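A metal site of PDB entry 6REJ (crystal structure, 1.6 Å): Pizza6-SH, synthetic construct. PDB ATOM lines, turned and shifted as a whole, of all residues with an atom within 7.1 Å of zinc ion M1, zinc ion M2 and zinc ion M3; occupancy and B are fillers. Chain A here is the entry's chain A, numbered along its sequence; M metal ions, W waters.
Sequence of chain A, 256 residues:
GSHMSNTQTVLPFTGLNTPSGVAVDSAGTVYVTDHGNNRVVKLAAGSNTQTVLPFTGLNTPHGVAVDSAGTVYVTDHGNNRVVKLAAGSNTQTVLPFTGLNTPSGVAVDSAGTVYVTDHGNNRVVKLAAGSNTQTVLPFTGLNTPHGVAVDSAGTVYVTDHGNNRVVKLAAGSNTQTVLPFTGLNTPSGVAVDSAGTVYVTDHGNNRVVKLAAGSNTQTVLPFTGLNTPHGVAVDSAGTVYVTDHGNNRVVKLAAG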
ATOM      1  N   PRO A  19       9.233 -18.940  34.621  1.00  0.00           N
ATOM      2  CA  PRO A  19       9.126 -20.405  34.548  1.00  0.00           C
ATOM      3  C   PRO A  19       9.447 -20.867  33.141  1.00  0.00           C
ATOM      4  O   PRO A  19       9.085 -20.211  32.157  1.00  0.00           O
ATOM      5  CB  PRO A  19       7.660 -20.669  34.908  1.00  0.00           C
ATOM      6  CG  PRO A  19       6.954 -19.432  34.429  1.00  0.00           C
ATOM      7  CD  PRO A  19       7.905 -18.287  34.630  1.00  0.00           C
ATOM      8  N   SER A  20      10.127 -21.999  33.037  1.00  0.00           N
ATOM      9  CA  SER A  20      10.665 -22.421  31.747  1.00  0.00           C
ATOM     10  C   SER A  20      10.176 -23.809  31.404  1.00  0.00           C
ATOM     11  O   SER A  20       9.213 -23.972  30.647  1.00  0.00           O
ATOM     12  CB  SER A  20      12.187 -22.378  31.754  1.00  0.00           C
ATOM     13  OG  SER A  20      12.695 -22.323  30.431  1.00  0.00           O
ATOM     14  N   GLY A  21      10.808 -24.829  31.978  1.00  0.00           N
ATOM     15  CA  GLY A  21      10.397 -26.186  31.724  1.00  0.00           C
ATOM     16  C   GLY A  21       9.246 -26.601  32.611  1.00  0.00           C
ATOM     17  O   GLY A  21       9.056 -26.099  33.712  1.00  0.00           O
ATOM     18  N   HIS A  35      13.507 -20.303  36.363  1.00  0.00           N
ATOM     19  CA  HIS A  35      14.752 -19.722  35.844  1.00  0.00           C
ATOM     20  C   HIS A  35      15.439 -18.767  36.801  1.00  0.00           C
ATOM     21  O   HIS A  35      16.544 -19.018  37.282  1.00  0.00           O
ATOM     22  CB  HIS A  35      14.487 -18.935  34.570  1.00  0.00           C
ATOM     23  CG  HIS A  35      14.759 -19.697  33.320  1.00  0.00           C
ATOM     24  ND1 HIS A  35      14.736 -19.102  32.075  1.00  0.00           N
ATOM     25  CD2 HIS A  35      15.021 -20.997  33.111  1.00  0.00           C
ATOM     26  CE1 HIS A  35      14.992 -20.018  31.154  1.00  0.00           C
ATOM     27  NE2 HIS A  35      15.154 -21.182  31.766  1.00  0.00           N
ATOM     28  N   HIS A  62      16.607 -25.288  33.133  1.00  0.00           N
ATOM     29  CA  HIS A  62      15.763 -25.143  31.955  1.00  0.00           C
ATOM     30  C   HIS A  62      14.719 -26.256  31.859  1.00  0.00           C
ATOM     31  O   HIS A  62      13.610 -26.044  32.226  1.00  0.00           O
ATOM     32  CB  HIS A  62      16.703 -25.191  30.791  1.00  0.00           C
ATOM     33  CG  HIS A  62      16.040 -24.484  29.710  1.00  0.00           C
ATOM     34  ND1 HIS A  62      16.124 -23.168  29.631  1.00  0.00           N
ATOM     35  CD2 HIS A  62      15.159 -24.910  28.795  1.00  0.00           C
ATOM     36  CE1 HIS A  62      15.403 -22.764  28.626  1.00  0.00           C
ATOM     37  NE2 HIS A  62      14.783 -23.813  28.113  1.00  0.00           N
ATOM     38  N   GLY A  63      15.129 -27.387  31.358  1.00  0.00           N
ATOM     39  CA  GLY A  63      14.217 -28.492  31.177  1.00  0.00           C
ATOM     40  C   GLY A  63      14.027 -29.318  32.446  1.00  0.00           C
ATOM     41  O   GLY A  63      14.877 -29.358  33.324  1.00  0.00           O
ATOM     42  N   HIS A  77      21.339 -25.621  32.713  1.00  0.00           N
ATOM     43  CA  HIS A  77      21.752 -24.871  31.523  1.00  0.00           C
ATOM     44  C   HIS A  77      23.116 -24.221  31.687  1.00  0.00           C
ATOM     45  O   HIS A  77      24.049 -24.491  30.906  1.00  0.00           O
ATOM     46  CB  HIS A  77      20.682 -23.804  31.273  1.00  0.00           C
ATOM     47  CG  HIS A  77      20.560 -23.346  29.860  1.00  0.00           C
ATOM     48  ND1 HIS A  77      21.214 -22.228  29.384  1.00  0.00           N
ATOM     49  CD2 HIS A  77      19.824 -23.821  28.820  1.00  0.00           C
ATOM     50  CE1 HIS A  77      20.893 -22.042  28.114  1.00  0.00           C
ATOM     51  NE2 HIS A  77      20.060 -22.999  27.753  1.00  0.00           N
ATOM     52  N   SER A 104      19.407 -28.030  27.272  1.00  0.00           N
ATOM     53  CA  SER A 104      18.126 -27.337  27.371  1.00  0.00           C
ATOM     54  C   SER A 104      17.012 -28.300  27.752  1.00  0.00           C
ATOM     55  O   SER A 104      16.594 -28.362  28.915  1.00  0.00           O
ATOM     56  CB  SER A 104      17.825 -26.639  26.047  1.00  0.00           C
ATOM     57  OG  SER A 104      16.815 -25.663  26.189  1.00  0.00           O
ATOM     58  N   GLY A 105      16.516 -29.053  26.789  1.00  0.00           N
ATOM     59  CA  GLY A 105      15.389 -29.940  27.042  1.00  0.00           C
ATOM     60  C   GLY A 105      15.877 -31.275  27.559  1.00  0.00           C
ATOM     61  O   GLY A 105      17.003 -31.677  27.331  1.00  0.00           O
ATOM     62  N   HIS A 119      21.943 -27.893  23.224  1.00  0.00           N
ATOM     63  CA  HIS A 119      21.634 -26.689  22.463  1.00  0.00           C
ATOM     64  C   HIS A 119      22.846 -26.140  21.728  1.00  0.00           C
ATOM     65  O   HIS A 119      22.826 -25.957  20.505  1.00  0.00           O
ATOM     66  CB  HIS A 119      21.079 -25.655  23.446  1.00  0.00           C
ATOM     67  CG  HIS A 119      20.133 -24.666  22.853  1.00  0.00           C
ATOM     68  ND1 HIS A 119      20.541 -23.423  22.424  1.00  0.00           N
ATOM     69  CD2 HIS A 119      18.787 -24.696  22.705  1.00  0.00           C
ATOM     70  CE1 HIS A 119      19.489 -22.744  21.995  1.00  0.00           C
ATOM     71  NE2 HIS A 119      18.411 -23.500  22.157  1.00  0.00           N
ATOM     72  N   THR A 144      19.866 -26.159  15.818  1.00  0.00           N
ATOM     73  CA  THR A 144      19.689 -25.907  17.255  1.00  0.00           C
ATOM     74  C   THR A 144      18.420 -26.555  17.790  1.00  0.00           C
ATOM     75  O   THR A 144      17.309 -26.045  17.605  1.00  0.00           O
ATOM     76  CB  THR A 144      19.717 -24.413  17.554  1.00  0.00           C
ATOM     77  OG1 THR A 144      20.918 -23.845  17.011  1.00  0.00           O
ATOM     78  CG2 THR A 144      19.701 -24.189  19.035  1.00  0.00           C
ATOM     79  N   PRO A 145      18.549 -27.692  18.460  1.00  0.00           N
ATOM     80  CA  PRO A 145      17.391 -28.349  19.069  1.00  0.00           C
ATOM     81  C   PRO A 145      17.076 -27.744  20.416  1.00  0.00           C
ATOM     82  O   PRO A 145      17.974 -27.326  21.157  1.00  0.00           O
ATOM     83  CB  PRO A 145      17.854 -29.804  19.202  1.00  0.00           C
ATOM     84  CG  PRO A 145      19.347 -29.660  19.468  1.00  0.00           C
ATOM     85  CD  PRO A 145      19.805 -28.446  18.682  1.00  0.00           C
ATOM     86  N   HIS A 146      15.802 -27.736  20.756  1.00  0.00           N
ATOM     87  CA  HIS A 146      15.413 -27.120  22.035  1.00  0.00           C
ATOM     88  C   HIS A 146      14.610 -28.105  22.896  1.00  0.00           C
ATOM     89  O   HIS A 146      15.123 -28.601  23.844  1.00  0.00           O
ATOM     90  CB  HIS A 146      14.633 -25.853  21.710  1.00  0.00           C
ATOM     91  CG  HIS A 146      14.370 -25.147  22.961  1.00  0.00           C
ATOM     92  ND1 HIS A 146      15.154 -24.117  23.372  1.00  0.00           N
ATOM     93  CD2 HIS A 146      13.531 -25.438  23.970  1.00  0.00           C
ATOM     94  CE1 HIS A 146      14.730 -23.716  24.555  1.00  0.00           C
ATOM     95  NE2 HIS A 146      13.735 -24.493  24.918  1.00  0.00           N
ATOM     96  N   GLY A 147      13.368 -28.333  22.565  1.00  0.00           N
ATOM     97  CA  GLY A 147      12.585 -29.280  23.334  1.00  0.00           C
ATOM     98  C   GLY A 147      12.794 -30.711  22.870  1.00  0.00           C
ATOM     99  O   GLY A 147      13.147 -30.950  21.722  1.00  0.00           O
ATOM    100  N   THR A 159      12.125 -30.303  18.952  1.00  0.00           N
ATOM    101  CA  THR A 159      11.869 -29.051  18.279  1.00  0.00           C
ATOM    102  C   THR A 159      13.170 -28.481  17.728  1.00  0.00           C
ATOM    103  O   THR A 159      14.188 -28.436  18.422  1.00  0.00           O
ATOM    104  CB  THR A 159      11.161 -28.049  19.200  1.00  0.00           C
ATOM    105  OG1 THR A 159      11.993 -27.710  20.321  1.00  0.00           O
ATOM    106  CG2 THR A 159       9.873 -28.638  19.714  1.00  0.00           C
ATOM    107  N   HIS A 161      14.813 -25.310  16.415  1.00  0.00           N
ATOM    108  CA  HIS A 161      14.635 -23.865  16.495  1.00  0.00           C
ATOM    109  C   HIS A 161      14.760 -23.193  15.130  1.00  0.00           C
ATOM    110  O   HIS A 161      13.827 -22.521  14.662  1.00  0.00           O
ATOM    111  CB  HIS A 161      15.671 -23.285  17.458  1.00  0.00           C
ATOM    112  CG  HIS A 161      15.171 -22.134  18.270  1.00  0.00           C
ATOM    113  ND1 HIS A 161      15.690 -20.864  18.153  1.00  0.00           N
ATOM    114  CD2 HIS A 161      14.211 -22.063  19.226  1.00  0.00           C
ATOM    115  CE1 HIS A 161      15.068 -20.059  18.994  1.00  0.00           C
ATOM    116  NE2 HIS A 161      14.169 -20.761  19.662  1.00  0.00           N
ATOM    117  N   PRO A 187       9.467 -23.000  17.365  1.00  0.00           N
ATOM    118  CA  PRO A 187       8.926 -23.988  18.307  1.00  0.00           C
ATOM    119  C   PRO A 187       9.933 -24.256  19.414  1.00  0.00           C
ATOM    120  O   PRO A 187      11.150 -24.318  19.192  1.00  0.00           O
ATOM    121  CB  PRO A 187       8.720 -25.226  17.439  1.00  0.00           C
ATOM    122  CG  PRO A 187       9.797 -25.103  16.392  1.00  0.00           C
ATOM    123  CD  PRO A 187       9.894 -23.613  16.102  1.00  0.00           C
ATOM    124  N   SER A 188       9.415 -24.421  20.627  1.00  0.00           N
ATOM    125  CA  SER A 188      10.270 -24.552  21.790  1.00  0.00           C
ATOM    126  C   SER A 188       9.992 -25.844  22.536  1.00  0.00           C
ATOM    127  O   SER A 188      10.646 -26.866  22.300  1.00  0.00           O
ATOM    128  CB  SER A 188      10.083 -23.347  22.708  1.00  0.00           C
ATOM    129  OG  SER A 188      10.872 -23.466  23.884  1.00  0.00           O
ATOM    130  N   GLY A 189       9.018 -25.813  23.440  1.00  0.00           N
ATOM    131  CA  GLY A 189       8.668 -27.018  24.175  1.00  0.00           C
ATOM    132  C   GLY A 189       7.904 -28.003  23.322  1.00  0.00           C
ATOM    133  O   GLY A 189       7.258 -27.648  22.332  1.00  0.00           O
ATOM    134  N   HIS A 203       6.717 -20.554  20.313  1.00  0.00           N
ATOM    135  CA  HIS A 203       7.260 -19.485  21.126  1.00  0.00           C
ATOM    136  C   HIS A 203       7.068 -18.124  20.467  1.00  0.00           C
ATOM    137  O   HIS A 203       6.644 -17.158  21.115  1.00  0.00           O
ATOM    138  CB  HIS A 203       8.740 -19.759  21.396  1.00  0.00           C
ATOM    139  CG  HIS A 203       9.340 -18.902  22.462  1.00  0.00           C
ATOM    140  ND1 HIS A 203       9.837 -17.640  22.205  1.00  0.00           N
ATOM    141  CD2 HIS A 203       9.595 -19.144  23.769  1.00  0.00           C
ATOM    142  CE1 HIS A 203      10.347 -17.134  23.319  1.00  0.00           C
ATOM    143  NE2 HIS A 203      10.203 -18.024  24.280  1.00  0.00           N
ATOM    144  N   ASN A 227       2.660 -14.945  26.230  1.00  0.00           N
ATOM    145  CA  ASN A 227       3.826 -14.150  25.879  1.00  0.00           C
ATOM    146  C   ASN A 227       5.052 -15.046  25.959  1.00  0.00           C
ATOM    147  O   ASN A 227       5.519 -15.368  27.060  1.00  0.00           O
ATOM    148  CB  ASN A 227       3.980 -12.946  26.810  1.00  0.00           C
ATOM    149  CG  ASN A 227       5.049 -11.986  26.341  1.00  0.00           C
ATOM    150  OD1 ASN A 227       5.432 -11.991  25.164  1.00  0.00           O
ATOM    151  ND2 ASN A 227       5.563 -11.160  27.247  1.00  0.00           N
ATOM    152  N   THR A 228       5.579 -15.437  24.806  1.00  0.00           N
ATOM    153  CA  THR A 228       6.702 -16.355  24.715  1.00  0.00           C
ATOM    154  C   THR A 228       6.495 -17.625  25.542  1.00  0.00           C
ATOM    155  O   THR A 228       7.281 -17.928  26.439  1.00  0.00           O
ATOM    156  CB  THR A 228       8.000 -15.657  25.120  1.00  0.00           C
ATOM    157  OG1 THR A 228       8.083 -15.591  26.553  1.00  0.00           O
ATOM    158  CG2 THR A 228       8.055 -14.249  24.543  1.00  0.00           C
ATOM    159  N   PRO A 229       5.453 -18.403  25.244  1.00  0.00           N
ATOM    160  CA  PRO A 229       5.269 -19.669  25.957  1.00  0.00           C
ATOM    161  C   PRO A 229       6.457 -20.578  25.694  1.00  0.00           C
ATOM    162  O   PRO A 229       6.979 -20.642  24.578  1.00  0.00           O
ATOM    163  CB  PRO A 229       3.978 -20.234  25.360  1.00  0.00           C
ATOM    164  CG  PRO A 229       3.962 -19.693  23.972  1.00  0.00           C
ATOM    165  CD  PRO A 229       4.539 -18.304  24.082  1.00  0.00           C
ATOM    166  N   HIS A 230       6.855 -21.282  26.735  1.00  0.00           N
ATOM    167  CA  HIS A 230       8.107 -22.048  26.663  1.00  0.00           C
ATOM    168  C   HIS A 230       7.912 -23.556  26.760  1.00  0.00           C
ATOM    169  O   HIS A 230       8.226 -24.214  25.833  1.00  0.00           O
ATOM    170  CB  HIS A 230       8.982 -21.628  27.826  1.00  0.00           C
ATOM    171  CG  HIS A 230      10.415 -21.875  27.541  1.00  0.00           C
ATOM    172  ND1 HIS A 230      11.148 -20.997  26.800  1.00  0.00           N
ATOM    173  CD2 HIS A 230      11.216 -22.908  27.807  1.00  0.00           C
ATOM    174  CE1 HIS A 230      12.381 -21.446  26.686  1.00  0.00           C
ATOM    175  NE2 HIS A 230      12.452 -22.598  27.334  1.00  0.00           N
ATOM    176  N   GLY A 231       7.485 -24.034  27.896  1.00  0.00           N
ATOM    177  CA  GLY A 231       7.362 -25.464  28.104  1.00  0.00           C
ATOM    178  C   GLY A 231       5.931 -25.927  27.990  1.00  0.00           C
ATOM    179  O   GLY A 231       4.995 -25.137  28.154  1.00  0.00           O
ATOM    180  N   THR A 243       4.148 -23.145  30.359  1.00  0.00           N
ATOM    181  CA  THR A 243       4.856 -22.094  31.070  1.00  0.00           C
ATOM    182  C   THR A 243       4.859 -20.835  30.220  1.00  0.00           C
ATOM    183  O   THR A 243       5.413 -20.820  29.106  1.00  0.00           O
ATOM    184  CB  THR A 243       6.276 -22.533  31.409  1.00  0.00           C
ATOM    185  OG1 THR A 243       6.920 -22.972  30.205  1.00  0.00           O
ATOM    186  CG2 THR A 243       6.234 -23.679  32.392  1.00  0.00           C
ATOM    187  N   HIS A 245       6.507 -17.940  29.885  1.00  0.00           N
ATOM    188  CA  HIS A 245       7.778 -17.352  30.274  1.00  0.00           C
ATOM    189  C   HIS A 245       7.669 -15.840  30.416  1.00  0.00           C
ATOM    190  O   HIS A 245       8.057 -15.270  31.445  1.00  0.00           O
ATOM    191  CB  HIS A 245       8.823 -17.764  29.215  1.00  0.00           C
ATOM    192  CG  HIS A 245      10.225 -17.344  29.515  1.00  0.00           C
ATOM    193  ND1 HIS A 245      10.729 -16.117  29.142  1.00  0.00           N
ATOM    194  CD2 HIS A 245      11.262 -18.036  30.050  1.00  0.00           C
ATOM    195  CE1 HIS A 245      12.005 -16.047  29.492  1.00  0.00           C
ATOM    196  NE2 HIS A 245      12.353 -17.196  30.044  1.00  0.00           N
ATOM    197  N   GLY A 246       7.085 -15.170  29.408  1.00  0.00           N
ATOM    198  CA  GLY A 246       7.026 -13.722  29.395  1.00  0.00           C
ATOM    199  C   GLY A 246       6.043 -13.123  30.379  1.00  0.00           C
ATOM    200  O   GLY A 246       6.168 -11.940  30.723  1.00  0.00           O
HETATM  201 ZN    ZN M   1      13.141 -24.583  26.880  1.00  0.00          ZN
HETATM  202 ZN    ZN M   2      11.394 -18.965  26.296  1.00  0.00          ZN
HETATM  203 ZN    ZN M   3      16.391 -22.715  22.411  1.00  0.00          ZN
HETATM  204 ZN    ZN M   4      13.686 -19.497  29.622  1.00  0.00          ZN
HETATM  205 ZN    ZN M   5      18.724 -23.059  26.034  1.00  0.00          ZN
HETATM  206  O   HOH W   1      13.804 -19.280  25.022  1.00  0.00           O
HETATM  207  O   HOH W   2      16.477 -20.814  23.462  1.00  0.00           O
HETATM  208  O   HOH W   3      11.768 -26.649  27.434  1.00  0.00           O
HETATM  209  O   HOH W   4      12.271 -16.292  25.599  1.00  0.00           O
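Ser 104 touches zinc ion M1. OG of Ser 188 touches zinc ion M1, 3.9 Å away.
ND1 of His 230 is bound to zinc ion M2 (2.1 Å). Zinc ion M2 is bound by NE2 of His 203 (2.5 Å). Slightly farther from zinc ion M2 lies water W1 (2.7 Å).
The backbone NH (N) of Gly 147 lies within hydrogen-bond range of the backbone carbonyl oxygen (O) of Ser 188 (3.1 Å). O of His 146 is in hydrogen-bond range of N of Gly 105 (3.3 Å). The backbone carbonyl oxygen (O) of His 230 is in hydrogen-bond range of the backbone NH (N) of Gly 189 (3.0 Å). The side-chain hydroxyl (OG) of Ser 188 sits close to a ring nitrogen (NE2) of His 146 (3.2 Å). A ring nitrogen (NE2) of His 62 sits close to the side-chain hydroxyl of Ser 20 (3.5 Å). The backbone NH (N) of His 146 is in hydrogen-bond range of the backbone carbonyl oxygen (O) of Thr 159. N of His 161 lies within hydrogen-bond range of O of Thr 144 (2.9 Å). O of His 62 lies within hydrogen-bond range of N of Gly 21, at 3.1 Å.
CD2 of His 161 touches zinc ion M3 (3.9 Å). Of the 28 residues printed, 3 come within 4 Å of zinc ion M3.
NE2 of His 146 binds zinc ion M1, 2.1 Å away. A ring nitrogen (NE2) of His 230 binds zinc ion M1 (2.1 Å). A ring nitrogen (NE2) of His 62 binds zinc ion M1 (2.2 Å). Water W3 is bound to zinc ion M1, 2.5 Å away. Zinc ion M1 has four donor atoms within binding distance.
ND1 of His 146 binds zinc ion M3, 2.1 Å away. Water W2 is bound to zinc ion M3. NE2 of His 119 binds zinc ion M3 (2.2 Å).
His 245 touches zinc ion M2. Of the 28 residues printed, 3 come within 4 Å of zinc ion M2. The nearest printed residue that does not touch zinc ion M2 is Thr 228 (4.2 Å).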
